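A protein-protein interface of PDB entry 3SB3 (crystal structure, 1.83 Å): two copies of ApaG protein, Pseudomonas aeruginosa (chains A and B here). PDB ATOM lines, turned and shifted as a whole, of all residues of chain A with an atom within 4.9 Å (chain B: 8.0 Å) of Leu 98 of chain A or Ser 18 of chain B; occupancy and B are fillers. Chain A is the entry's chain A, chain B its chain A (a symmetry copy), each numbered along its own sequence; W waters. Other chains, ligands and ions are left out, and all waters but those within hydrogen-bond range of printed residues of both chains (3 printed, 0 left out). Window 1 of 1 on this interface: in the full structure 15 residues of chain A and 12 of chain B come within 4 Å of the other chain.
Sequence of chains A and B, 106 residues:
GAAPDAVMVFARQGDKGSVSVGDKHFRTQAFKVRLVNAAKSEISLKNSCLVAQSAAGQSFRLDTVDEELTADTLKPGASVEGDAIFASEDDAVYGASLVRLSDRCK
The backbone NH (N) of Val 9 of chain A sits at hydrogen-bond distance from the backbone carbonyl oxygen (O) of Ser 20 of chain B, at 2.8 Å. The backbone NH (N) of Val 99 of chain A sits at hydrogen-bond distance from the side-chain hydroxyl (OG) of Ser 18 of chain B (3.4 Å). O of Ala 11 of chain A lies within hydrogen-bond range of N of Ser 18 of chain B, at 2.9 Å. The backbone carbonyl oxygen (O) of Ser 97 of chain A lies within hydrogen-bond range of the side-chain hydroxyl (OH) of Tyr 94 of chain B (3.3 Å). The side-chain hydroxyl (OG) of Ser 97 of chain A is in hydrogen-bond range of the guanidinium group (NE) of Arg 27 of chain B, 2.9 Å away.
The side-chain hydroxyl (OG) of Ser 20 of chain B lies within hydrogen-bond range of a ring nitrogen (ND1) of His 25 of chain B (2.9 Å). The side-chain hydroxyl of Tyr 94 of chain B is in hydrogen-bond range of the backbone carbonyl oxygen of Gly 17 of chain B. The guanidinium group of Arg 100 of chain A is in hydrogen-bond range of the side-chain amide oxygen of Gln 53 of chain A, 3.0 Å away. The backbone NH (N) of Phe 26 of chain B sits at hydrogen-bond distance from the backbone carbonyl oxygen (O) of Val 19 of chain B. N of Val 51 of chain A lies within hydrogen-bond range of O of Arg 100 of chain A. The backbone carbonyl oxygen of Ser 88 of chain B is in hydrogen-bond range of the backbone NH of Arg 27 of chain B (2.8 Å).
CD1 of Phe 10 of chain A touches CG2 of Val 19 of chain B, 3.9 Å away. Ala 11 of chain A touches Gly 17 of chain B. Arg 27 of chain B touches Gln 53 of chain A. O of Ser 97 of chain A touches O of Gly 17 of chain B, 3.9 Å away. CB of Ser 18 of chain B touches O of Ser 97 of chain A (3.4 Å). CA of Leu 98 of chain A touches OG of Ser 18 of chain B, at 3.5 Å. Leu 98 of chain A touches His 25 of chain B. Arg 27 of chain B touches Leu 98 of chain A (NH2 to CB, 3.5 Å). Val 99 of chain A touches Ser 20 of chain B (O to CB, 3.6 Å). Ser 20 of chain B touches Arg 100 of chain A (OG to CB, 3.6 Å).
Leu 98 of chain A touches just these residues of chain B: Ser 18 (3.5 Å), His 25 (3.5 Å) and Arg 27 (3.5 Å). Of the printed residues of chain A, Ser 18 of chain B touches Phe 10, Ala 11, Ser 97, Leu 98 and Val 99. Of the printed residues of chain B, Gln 53 of chain A touches Arg 27. Printed residues of chain A within 4 Å of Val 19 of chain B: Val 9 (3.4 Å) and Phe 10 (3.9 Å). Of the printed residues of chain B, Phe 10 of chain A touches Ser 18 (3.7 Å) and Val 19 (3.9 Å). Of the printed residues of chain A, Gly 17 of chain B touches Ala 11 (3.1 Å) and Ser 97 (3.9 Å). Of the printed residues of chain B, Arg 100 of chain A touches Ser 20 and His 25. Phe 26 of chain B touches none of the printed residues of chain A. Lys 16 of chain B touches none of the printed residues of chain A. The nearest residue of chain B that does not touch Leu 98 of chain A is Ser 20 of chain B (4.1 Å). The nearest printed residue of chain A that does not touch Ser 18 of chain B is Val 9 of chain A (4.002 Å).
Of the 12 printed residues of chain A, 8 touch a printed residue of chain B. Printed residues of chain A that touch a printed residue of chain B: Val 9, Phe 10, Ala 11, Gln 53, Ser 97, Leu 98, Val 99 and Arg 100. Along chain A the printed residues that touch a printed residue of chain B span positions 9 to 100. Of the 20 printed residues of chain B, 7 touch a printed residue of chain A. Printed residues of chain B that touch a printed residue of chain A: Gly 17, Ser 18, Val 19, Ser 20, His 25, Arg 27 and Tyr 94. Hydrophobic or aromatic side chains of chain B within 4 Å of the printed part of chain A: Val 19, His 25 and Tyr 94. Among the printed residues, no Asp or Glu carboxylate lies within 4 Å of a Lys or Arg side-chain nitrogen of the other chain.
No position is printed for both chains. Of the 18 pairs that touch across the chains among the printed residues, none has its exchanged pair printed and touching as well.
Water W1 lies within hydrogen-bond range of OG of Ser 18 of chain B (2.6 Å), O of Val 99 of chain A (2.7 Å) and O of Val 9 of chain A (2.9 Å). Water W2 bridges the backbone carbonyl oxygen of Gly 22 of chain B and the guanidinium group of Arg 100 of chain A. Water W3 bridges the side-chain hydroxyl (OG) of Ser 18 of chain B (3.0 Å) and the backbone carbonyl oxygen (O) of Ser 97 of chain A (3.2 Å).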
ATOM      1  N   VAL A   9     -21.492  15.914  27.029  1.00  0.00           N
ATOM      2  CA  VAL A   9     -21.187  16.050  25.568  1.00  0.00           C
ATOM      3  C   VAL A   9     -22.489  16.350  24.812  1.00  0.00           C
ATOM      4  O   VAL A   9     -23.394  15.511  24.782  1.00  0.00           O
ATOM      5  CB  VAL A   9     -20.526  14.758  24.983  1.00  0.00           C
ATOM      6  CG1 VAL A   9     -20.022  15.036  23.557  1.00  0.00           C
ATOM      7  CG2 VAL A   9     -19.353  14.290  25.902  1.00  0.00           C
ATOM      8  N   PHE A  10     -22.583  17.562  24.234  1.00  0.00           N
ATOM      9  CA  PHE A  10     -23.703  18.003  23.426  1.00  0.00           C
ATOM     10  C   PHE A  10     -23.210  18.047  22.003  1.00  0.00           C
ATOM     11  O   PHE A  10     -22.162  18.635  21.761  1.00  0.00           O
ATOM     12  CB  PHE A  10     -24.161  19.393  23.864  1.00  0.00           C
ATOM     13  CG  PHE A  10     -24.712  19.431  25.268  1.00  0.00           C
ATOM     14  CD1 PHE A  10     -26.063  19.202  25.491  1.00  0.00           C
ATOM     15  CD2 PHE A  10     -23.892  19.689  26.339  1.00  0.00           C
ATOM     16  CE1 PHE A  10     -26.582  19.202  26.788  1.00  0.00           C
ATOM     17  CE2 PHE A  10     -24.379  19.717  27.645  1.00  0.00           C
ATOM     18  CZ  PHE A  10     -25.745  19.465  27.873  1.00  0.00           C
ATOM     19  N   ALA A  11     -23.916  17.402  21.080  1.00  0.00           N
ATOM     20  CA  ALA A  11     -23.568  17.394  19.639  1.00  0.00           C
ATOM     21  C   ALA A  11     -24.780  17.686  18.779  1.00  0.00           C
ATOM     22  O   ALA A  11     -25.912  17.336  19.159  1.00  0.00           O
ATOM     23  CB  ALA A  11     -22.970  16.079  19.190  1.00  0.00           C
ATOM     24  N   PHE A  31     -20.050  17.372  13.169  1.00  0.00           N
ATOM     25  CA  PHE A  31     -20.881  17.737  14.317  1.00  0.00           C
ATOM     26  C   PHE A  31     -20.337  19.006  14.983  1.00  0.00           C
ATOM     27  O   PHE A  31     -19.129  19.179  15.059  1.00  0.00           O
ATOM     28  CB  PHE A  31     -20.830  16.668  15.392  1.00  0.00           C
ATOM     29  CG  PHE A  31     -21.360  15.326  14.967  1.00  0.00           C
ATOM     30  CD1 PHE A  31     -20.536  14.447  14.302  1.00  0.00           C
ATOM     31  CD2 PHE A  31     -22.658  14.954  15.259  1.00  0.00           C
ATOM     32  CE1 PHE A  31     -20.997  13.194  13.909  1.00  0.00           C
ATOM     33  CE2 PHE A  31     -23.122  13.712  14.908  1.00  0.00           C
ATOM     34  CZ  PHE A  31     -22.290  12.834  14.193  1.00  0.00           C
ATOM     35  N   VAL A  51     -15.632  10.078  20.168  1.00  0.00           N
ATOM     36  CA  VAL A  51     -16.018   8.968  19.299  1.00  0.00           C
ATOM     37  C   VAL A  51     -17.451   9.283  18.826  1.00  0.00           C
ATOM     38  O   VAL A  51     -18.306   9.712  19.614  1.00  0.00           O
ATOM     39  CB  VAL A  51     -16.003   7.639  20.104  1.00  0.00           C
ATOM     40  CG1 VAL A  51     -16.588   6.481  19.298  1.00  0.00           C
ATOM     41  CG2 VAL A  51     -14.596   7.309  20.564  1.00  0.00           C
ATOM     42  N   ALA A  52     -17.687   9.104  17.525  1.00  0.00           N
ATOM     43  CA  ALA A  52     -19.024   9.177  16.956  1.00  0.00           C
ATOM     44  C   ALA A  52     -19.470   7.764  16.619  1.00  0.00           C
ATOM     45  O   ALA A  52     -18.664   6.917  16.212  1.00  0.00           O
ATOM     46  CB  ALA A  52     -19.069  10.053  15.771  1.00  0.00           C
ATOM     47  N   GLN A  53     -20.749   7.499  16.787  1.00  0.00           N
ATOM     48  CA  GLN A  53     -21.271   6.140  16.583  1.00  0.00           C
ATOM     49  C   GLN A  53     -22.747   6.110  16.256  1.00  0.00           C
ATOM     50  O   GLN A  53     -23.493   7.061  16.509  1.00  0.00           O
ATOM     51  CB  GLN A  53     -20.962   5.254  17.785  1.00  0.00           C
ATOM     52  CG  GLN A  53     -21.671   5.654  19.042  1.00  0.00           C
ATOM     53  CD  GLN A  53     -21.084   4.998  20.262  1.00  0.00           C
ATOM     54  OE1 GLN A  53     -19.877   4.908  20.405  1.00  0.00           O
ATOM     55  NE2 GLN A  53     -21.917   4.532  21.128  1.00  0.00           N
ATOM     56  N   ALA A  96     -23.969   7.960  11.918  1.00  0.00           N
ATOM     57  CA  ALA A  96     -23.429   8.320  13.217  1.00  0.00           C
ATOM     58  C   ALA A  96     -24.438   9.322  13.788  1.00  0.00           C
ATOM     59  O   ALA A  96     -24.750  10.314  13.159  1.00  0.00           O
ATOM     60  CB  ALA A  96     -22.043   8.921  13.095  1.00  0.00           C
ATOM     61  N   SER A  97     -24.932   9.041  14.994  1.00  0.00           N
ATOM     62  CA  SER A  97     -25.959   9.839  15.632  1.00  0.00           C
ATOM     63  C   SER A  97     -25.641  10.282  17.047  1.00  0.00           C
ATOM     64  O   SER A  97     -26.483  10.946  17.676  1.00  0.00           O
ATOM     65  CB  SER A  97     -27.286   9.062  15.646  1.00  0.00           C
ATOM     66  OG  SER A  97     -27.143   7.842  16.310  1.00  0.00           O
ATOM     67  N   LEU A  98     -24.441   9.995  17.522  1.00  0.00           N
ATOM     68  CA  LEU A  98     -24.042  10.259  18.887  1.00  0.00           C
ATOM     69  C   LEU A  98     -22.567  10.586  18.907  1.00  0.00           C
ATOM     70  O   LEU A  98     -21.787   9.883  18.283  1.00  0.00           O
ATOM     71  CB  LEU A  98     -24.251   9.030  19.722  1.00  0.00           C
ATOM     72  CG  LEU A  98     -23.708   9.106  21.187  1.00  0.00           C
ATOM     73  CD1 LEU A  98     -24.505  10.155  21.994  1.00  0.00           C
ATOM     74  CD2 LEU A  98     -23.740   7.703  21.781  1.00  0.00           C
ATOM     75  N   VAL A  99     -22.196  11.658  19.591  1.00  0.00           N
ATOM     76  CA  VAL A  99     -20.813  11.899  19.941  1.00  0.00           C
ATOM     77  C   VAL A  99     -20.673  11.722  21.469  1.00  0.00           C
ATOM     78  O   VAL A  99     -21.506  12.242  22.264  1.00  0.00           O
ATOM     79  CB  VAL A  99     -20.307  13.308  19.477  1.00  0.00           C
ATOM     80  CG1 VAL A  99     -18.844  13.516  19.898  1.00  0.00           C
ATOM     81  CG2 VAL A  99     -20.506  13.464  17.937  1.00  0.00           C
ATOM     82  N   ARG A 100     -19.645  10.984  21.872  1.00  0.00           N
ATOM     83  CA  ARG A 100     -19.389  10.651  23.285  1.00  0.00           C
ATOM     84  C   ARG A 100     -17.910  10.613  23.554  1.00  0.00           C
ATOM     85  O   ARG A 100     -17.099  10.538  22.631  1.00  0.00           O
ATOM     86  CB  ARG A 100     -20.047   9.316  23.655  1.00  0.00           C
ATOM     87  CG  ARG A 100     -19.623   8.189  22.722  1.00  0.00           C
ATOM     88  CD  ARG A 100     -20.078   6.825  23.209  1.00  0.00           C
ATOM     89  NE  ARG A 100     -19.046   6.356  24.090  1.00  0.00           N
ATOM     90  CZ  ARG A 100     -18.036   5.529  23.776  1.00  0.00           C
ATOM     91  NH1 ARG A 100     -17.939   4.897  22.640  1.00  0.00           N
ATOM     92  NH2 ARG A 100     -17.167   5.257  24.720  1.00  0.00           N
ATOM     93  N   ASP B  15     -32.903  20.840  13.915  1.00  0.00           N
ATOM     94  CA  ASP B  15     -31.652  20.099  14.116  1.00  0.00           C
ATOM     95  C   ASP B  15     -31.786  18.751  14.772  1.00  0.00           C
ATOM     96  O   ASP B  15     -32.597  18.587  15.681  1.00  0.00           O
ATOM     97  CB  ASP B  15     -30.710  20.920  14.987  1.00  0.00           C
ATOM     98  CG  ASP B  15     -30.219  22.180  14.280  1.00  0.00           C
ATOM     99  OD1 ASP B  15     -30.145  22.182  13.018  1.00  0.00           O
ATOM    100  OD2 ASP B  15     -29.941  23.138  15.018  1.00  0.00           O
ATOM    101  N   LYS B  16     -30.909  17.848  14.350  1.00  0.00           N
ATOM    102  CA  LYS B  16     -30.727  16.533  14.925  1.00  0.00           C
ATOM    103  C   LYS B  16     -29.454  16.564  15.726  1.00  0.00           C
ATOM    104  O   LYS B  16     -28.432  17.176  15.324  1.00  0.00           O
ATOM    105  CB  LYS B  16     -30.589  15.445  13.839  1.00  0.00           C
ATOM    106  CG  LYS B  16     -31.786  15.261  12.941  1.00  0.00           C
ATOM    107  CD  LYS B  16     -31.470  14.313  11.793  1.00  0.00           C
ATOM    108  CE  LYS B  16     -32.678  13.923  10.908  1.00  0.00           C
ATOM    109  NZ  LYS B  16     -33.913  14.801  10.894  1.00  0.00           N
ATOM    110  N   GLY B  17     -29.483  15.867  16.856  1.00  0.00           N
ATOM    111  CA  GLY B  17     -28.388  15.983  17.822  1.00  0.00           C
ATOM    112  C   GLY B  17     -28.323  14.836  18.804  1.00  0.00           C
ATOM    113  O   GLY B  17     -28.979  13.802  18.601  1.00  0.00           O
ATOM    114  N   SER B  18     -27.497  15.041  19.831  1.00  0.00           N
ATOM    115  CA  SER B  18     -27.334  14.038  20.869  1.00  0.00           C
ATOM    116  C   SER B  18     -26.842  14.684  22.130  1.00  0.00           C
ATOM    117  O   SER B  18     -26.367  15.823  22.121  1.00  0.00           O
ATOM    118  CB  SER B  18     -26.391  12.923  20.468  1.00  0.00           C
ATOM    119  OG  SER B  18     -25.046  13.365  20.254  1.00  0.00           O
ATOM    120  N   VAL B  19     -27.077  13.974  23.221  1.00  0.00           N
ATOM    121  CA  VAL B  19     -26.562  14.331  24.539  1.00  0.00           C
ATOM    122  C   VAL B  19     -25.977  13.058  25.186  1.00  0.00           C
ATOM    123  O   VAL B  19     -26.661  12.014  25.241  1.00  0.00           O
ATOM    124  CB  VAL B  19     -27.687  14.931  25.472  1.00  0.00           C
ATOM    125  CG1 VAL B  19     -27.115  15.274  26.887  1.00  0.00           C
ATOM    126  CG2 VAL B  19     -28.404  16.161  24.778  1.00  0.00           C
ATOM    127  N   SER B  20     -24.758  13.168  25.725  1.00  0.00           N
ATOM    128  CA  SER B  20     -24.067  12.096  26.397  1.00  0.00           C
ATOM    129  C   SER B  20     -23.441  12.550  27.720  1.00  0.00           C
ATOM    130  O   SER B  20     -22.845  13.627  27.802  1.00  0.00           O
ATOM    131  CB  SER B  20     -22.955  11.501  25.500  1.00  0.00           C
ATOM    132  OG  SER B  20     -22.310  10.417  26.166  1.00  0.00           O
ATOM    133  N   VAL B  21     -23.603  11.724  28.747  1.00  0.00           N
ATOM    134  CA  VAL B  21     -23.041  11.944  30.083  1.00  0.00           C
ATOM    135  C   VAL B  21     -22.587  10.590  30.598  1.00  0.00           C
ATOM    136  O   VAL B  21     -23.447   9.782  30.881  1.00  0.00           O
ATOM    137  CB  VAL B  21     -24.133  12.450  31.069  1.00  0.00           C
ATOM    138  CG1 VAL B  21     -23.509  12.782  32.429  1.00  0.00           C
ATOM    139  CG2 VAL B  21     -24.940  13.626  30.464  1.00  0.00           C
ATOM    140  N   GLY B  22     -21.280  10.338  30.691  1.00  0.00           N
ATOM    141  CA  GLY B  22     -20.782   9.010  31.082  1.00  0.00           C
ATOM    142  C   GLY B  22     -21.259   8.079  30.001  1.00  0.00           C
ATOM    143  O   GLY B  22     -21.050   8.380  28.811  1.00  0.00           O
ATOM    144  N   ASP B  23     -21.957   7.005  30.360  1.00  0.00           N
ATOM    145  CA  ASP B  23     -22.466   6.082  29.326  1.00  0.00           C
ATOM    146  C   ASP B  23     -23.972   6.207  29.109  1.00  0.00           C
ATOM    147  O   ASP B  23     -24.573   5.329  28.514  1.00  0.00           O
ATOM    148  CB  ASP B  23     -22.013   4.630  29.530  1.00  0.00           C
ATOM    149  CG  ASP B  23     -22.465   4.014  30.794  1.00  0.00           C
ATOM    150  OD1 ASP B  23     -23.483   4.464  31.378  1.00  0.00           O
ATOM    151  OD2 ASP B  23     -21.803   2.969  31.208  1.00  0.00           O
ATOM    152  N   LYS B  24     -24.547   7.319  29.569  1.00  0.00           N
ATOM    153  CA  LYS B  24     -25.938   7.592  29.364  1.00  0.00           C
ATOM    154  C   LYS B  24     -26.040   8.482  28.132  1.00  0.00           C
ATOM    155  O   LYS B  24     -25.597   9.654  28.148  1.00  0.00           O
ATOM    156  CB  LYS B  24     -26.534   8.313  30.567  1.00  0.00           C
ATOM    157  CG  LYS B  24     -28.025   8.711  30.397  1.00  0.00           C
ATOM    158  CD  LYS B  24     -28.527   9.501  31.640  1.00  0.00           C
ATOM    159  CE  LYS B  24     -30.014   9.912  31.551  1.00  0.00           C
ATOM    160  NZ  LYS B  24     -30.261  10.791  30.376  1.00  0.00           N
ATOM    161  N   HIS B  25     -26.665   7.941  27.091  1.00  0.00           N
ATOM    162  CA  HIS B  25     -26.753   8.640  25.800  1.00  0.00           C
ATOM    163  C   HIS B  25     -28.180   8.816  25.343  1.00  0.00           C
ATOM    164  O   HIS B  25     -29.026   7.933  25.550  1.00  0.00           O
ATOM    165  CB  HIS B  25     -26.024   7.846  24.712  1.00  0.00           C
ATOM    166  CG  HIS B  25     -24.731   7.223  25.135  1.00  0.00           C
ATOM    167  ND1 HIS B  25     -23.655   7.958  25.572  1.00  0.00           N
ATOM    168  CD2 HIS B  25     -24.306   5.938  25.073  1.00  0.00           C
ATOM    169  CE1 HIS B  25     -22.629   7.154  25.795  1.00  0.00           C
ATOM    170  NE2 HIS B  25     -23.006   5.911  25.532  1.00  0.00           N
ATOM    171  N   PHE B  26     -28.477   9.941  24.697  1.00  0.00           N
ATOM    172  CA  PHE B  26     -29.712   9.979  23.910  1.00  0.00           C
ATOM    173  C   PHE B  26     -29.561  10.880  22.662  1.00  0.00           C
ATOM    174  O   PHE B  26     -28.658  11.735  22.569  1.00  0.00           O
ATOM    175  CB  PHE B  26     -30.958  10.340  24.769  1.00  0.00           C
ATOM    176  CG  PHE B  26     -30.925  11.692  25.425  1.00  0.00           C
ATOM    177  CD1 PHE B  26     -31.379  12.828  24.753  1.00  0.00           C
ATOM    178  CD2 PHE B  26     -30.525  11.819  26.750  1.00  0.00           C
ATOM    179  CE1 PHE B  26     -31.347  14.082  25.355  1.00  0.00           C
ATOM    180  CE2 PHE B  26     -30.511  13.034  27.366  1.00  0.00           C
ATOM    181  CZ  PHE B  26     -30.912  14.181  26.689  1.00  0.00           C
ATOM    182  N   ARG B  27     -30.448  10.646  21.710  1.00  0.00           N
ATOM    183  CA  ARG B  27     -30.548  11.424  20.496  1.00  0.00           C
ATOM    184  C   ARG B  27     -31.693  12.417  20.599  1.00  0.00           C
ATOM    185  O   ARG B  27     -32.664  12.179  21.325  1.00  0.00           O
ATOM    186  CB  ARG B  27     -30.823  10.497  19.309  1.00  0.00           C
ATOM    187  CG  ARG B  27     -29.584   9.736  18.786  1.00  0.00           C
ATOM    188  CD  ARG B  27     -29.092   8.644  19.742  1.00  0.00           C
ATOM    189  NE  ARG B  27     -27.992   7.907  19.114  1.00  0.00           N
ATOM    190  CZ  ARG B  27     -27.375   6.858  19.656  1.00  0.00           C
ATOM    191  NH1 ARG B  27     -27.775   6.374  20.836  1.00  0.00           N
ATOM    192  NH2 ARG B  27     -26.349   6.300  19.009  1.00  0.00           N
ATOM    193  N   THR B  28     -31.540  13.552  19.921  1.00  0.00           N
ATOM    194  CA  THR B  28     -32.517  14.628  19.983  1.00  0.00           C
ATOM    195  C   THR B  28     -32.951  15.033  18.549  1.00  0.00           C
ATOM    196  O   THR B  28     -32.149  14.994  17.593  1.00  0.00           O
ATOM    197  CB  THR B  28     -32.000  15.882  20.725  1.00  0.00           C
ATOM    198  OG1 THR B  28     -30.848  16.362  20.055  1.00  0.00           O
ATOM    199  CG2 THR B  28     -31.676  15.628  22.225  1.00  0.00           C
ATOM    200  N   GLN B  29     -34.225  15.392  18.425  1.00  0.00           N
ATOM    201  CA  GLN B  29     -34.819  16.036  17.240  1.00  0.00           C
ATOM    202  C   GLN B  29     -35.530  17.289  17.704  1.00  0.00           C
ATOM    203  O   GLN B  29     -36.523  17.239  18.490  1.00  0.00           O
ATOM    204  CB  GLN B  29     -35.807  15.091  16.556  1.00  0.00           C
ATOM    205  CG  GLN B  29     -36.572  15.672  15.340  1.00  0.00           C
ATOM    206  CD  GLN B  29     -35.667  15.975  14.214  1.00  0.00           C
ATOM    207  OE1 GLN B  29     -35.087  15.071  13.591  1.00  0.00           O
ATOM    208  NE2 GLN B  29     -35.467  17.248  13.963  1.00  0.00           N
ATOM    209  N   ILE B  85     -37.721  20.168  21.891  1.00  0.00           N
ATOM    210  CA  ILE B  85     -36.697  19.155  21.574  1.00  0.00           C
ATOM    211  C   ILE B  85     -37.051  17.803  22.205  1.00  0.00           C
ATOM    212  O   ILE B  85     -37.111  17.663  23.435  1.00  0.00           O
ATOM    213  CB  ILE B  85     -35.299  19.586  22.055  1.00  0.00           C
ATOM    214  CG1 ILE B  85     -34.782  20.813  21.279  1.00  0.00           C
ATOM    215  CG2 ILE B  85     -34.322  18.440  21.891  1.00  0.00           C
ATOM    216  CD1 ILE B  85     -33.461  21.449  21.839  1.00  0.00           C
ATOM    217  N   SER B  88     -34.980  10.215  22.134  1.00  0.00           N
ATOM    218  CA  SER B  88     -34.978   8.765  22.276  1.00  0.00           C
ATOM    219  C   SER B  88     -33.582   8.272  22.676  1.00  0.00           C
ATOM    220  O   SER B  88     -32.540   8.890  22.362  1.00  0.00           O
ATOM    221  CB  SER B  88     -35.459   8.092  20.990  1.00  0.00           C
ATOM    222  OG  SER B  88     -34.639   8.358  19.850  1.00  0.00           O
ATOM    223  N   GLU B  89     -33.546   7.080  23.268  1.00  0.00           N
ATOM    224  CA  GLU B  89     -32.252   6.537  23.680  1.00  0.00           C
ATOM    225  C   GLU B  89     -31.480   6.118  22.439  1.00  0.00           C
ATOM    226  O   GLU B  89     -30.277   6.381  22.311  1.00  0.00           O
ATOM    227  CB  GLU B  89     -32.451   5.349  24.633  1.00  0.00           C
ATOM    228  CG  GLU B  89     -32.927   5.757  26.005  1.00  0.00           C
ATOM    229  CD  GLU B  89     -33.025   4.567  26.974  1.00  0.00           C
ATOM    230  OE1 GLU B  89     -31.977   4.149  27.524  1.00  0.00           O
ATOM    231  OE2 GLU B  89     -34.163   4.087  27.188  1.00  0.00           O
ATOM    232  N   ASP B  91     -31.906   5.849  17.893  1.00  0.00           N
ATOM    233  CA  ASP B  91     -32.113   6.896  16.886  1.00  0.00           C
ATOM    234  C   ASP B  91     -33.570   6.936  16.351  1.00  0.00           C
ATOM    235  O   ASP B  91     -33.853   7.620  15.356  1.00  0.00           O
ATOM    236  CB  ASP B  91     -31.020   6.903  15.791  1.00  0.00           C
ATOM    237  CG  ASP B  91     -31.047   5.692  14.904  1.00  0.00           C
ATOM    238  OD1 ASP B  91     -31.890   4.818  15.141  1.00  0.00           O
ATOM    239  OD2 ASP B  91     -30.206   5.610  13.971  1.00  0.00           O
ATOM    240  N   TYR B  94     -35.502  10.269  15.218  1.00  0.00           N
ATOM    241  CA  TYR B  94     -35.230  10.907  13.946  1.00  0.00           C
ATOM    242  C   TYR B  94     -36.346  10.687  12.975  1.00  0.00           C
ATOM    243  O   TYR B  94     -36.432  11.412  11.979  1.00  0.00           O
ATOM    244  CB  TYR B  94     -33.841  10.512  13.351  1.00  0.00           C
ATOM    245  CG  TYR B  94     -32.636  10.990  14.186  1.00  0.00           C
ATOM    246  CD1 TYR B  94     -32.711  12.031  15.108  1.00  0.00           C
ATOM    247  CD2 TYR B  94     -31.413  10.426  14.006  1.00  0.00           C
ATOM    248  CE1 TYR B  94     -31.580  12.453  15.852  1.00  0.00           C
ATOM    249  CE2 TYR B  94     -30.279  10.859  14.728  1.00  0.00           C
ATOM    250  CZ  TYR B  94     -30.365  11.851  15.672  1.00  0.00           C
ATOM    251  OH  TYR B  94     -29.181  12.243  16.339  1.00  0.00           O
HETATM  252  O   HOH W   1     -23.536  13.995  22.289  1.00  0.00           O
HETATM  253  O   HOH W   2     -19.136   7.596  26.965  1.00  0.00           O
HETATM  254  O   HOH W   3     -25.433  13.900  17.338  1.00  0.00           O
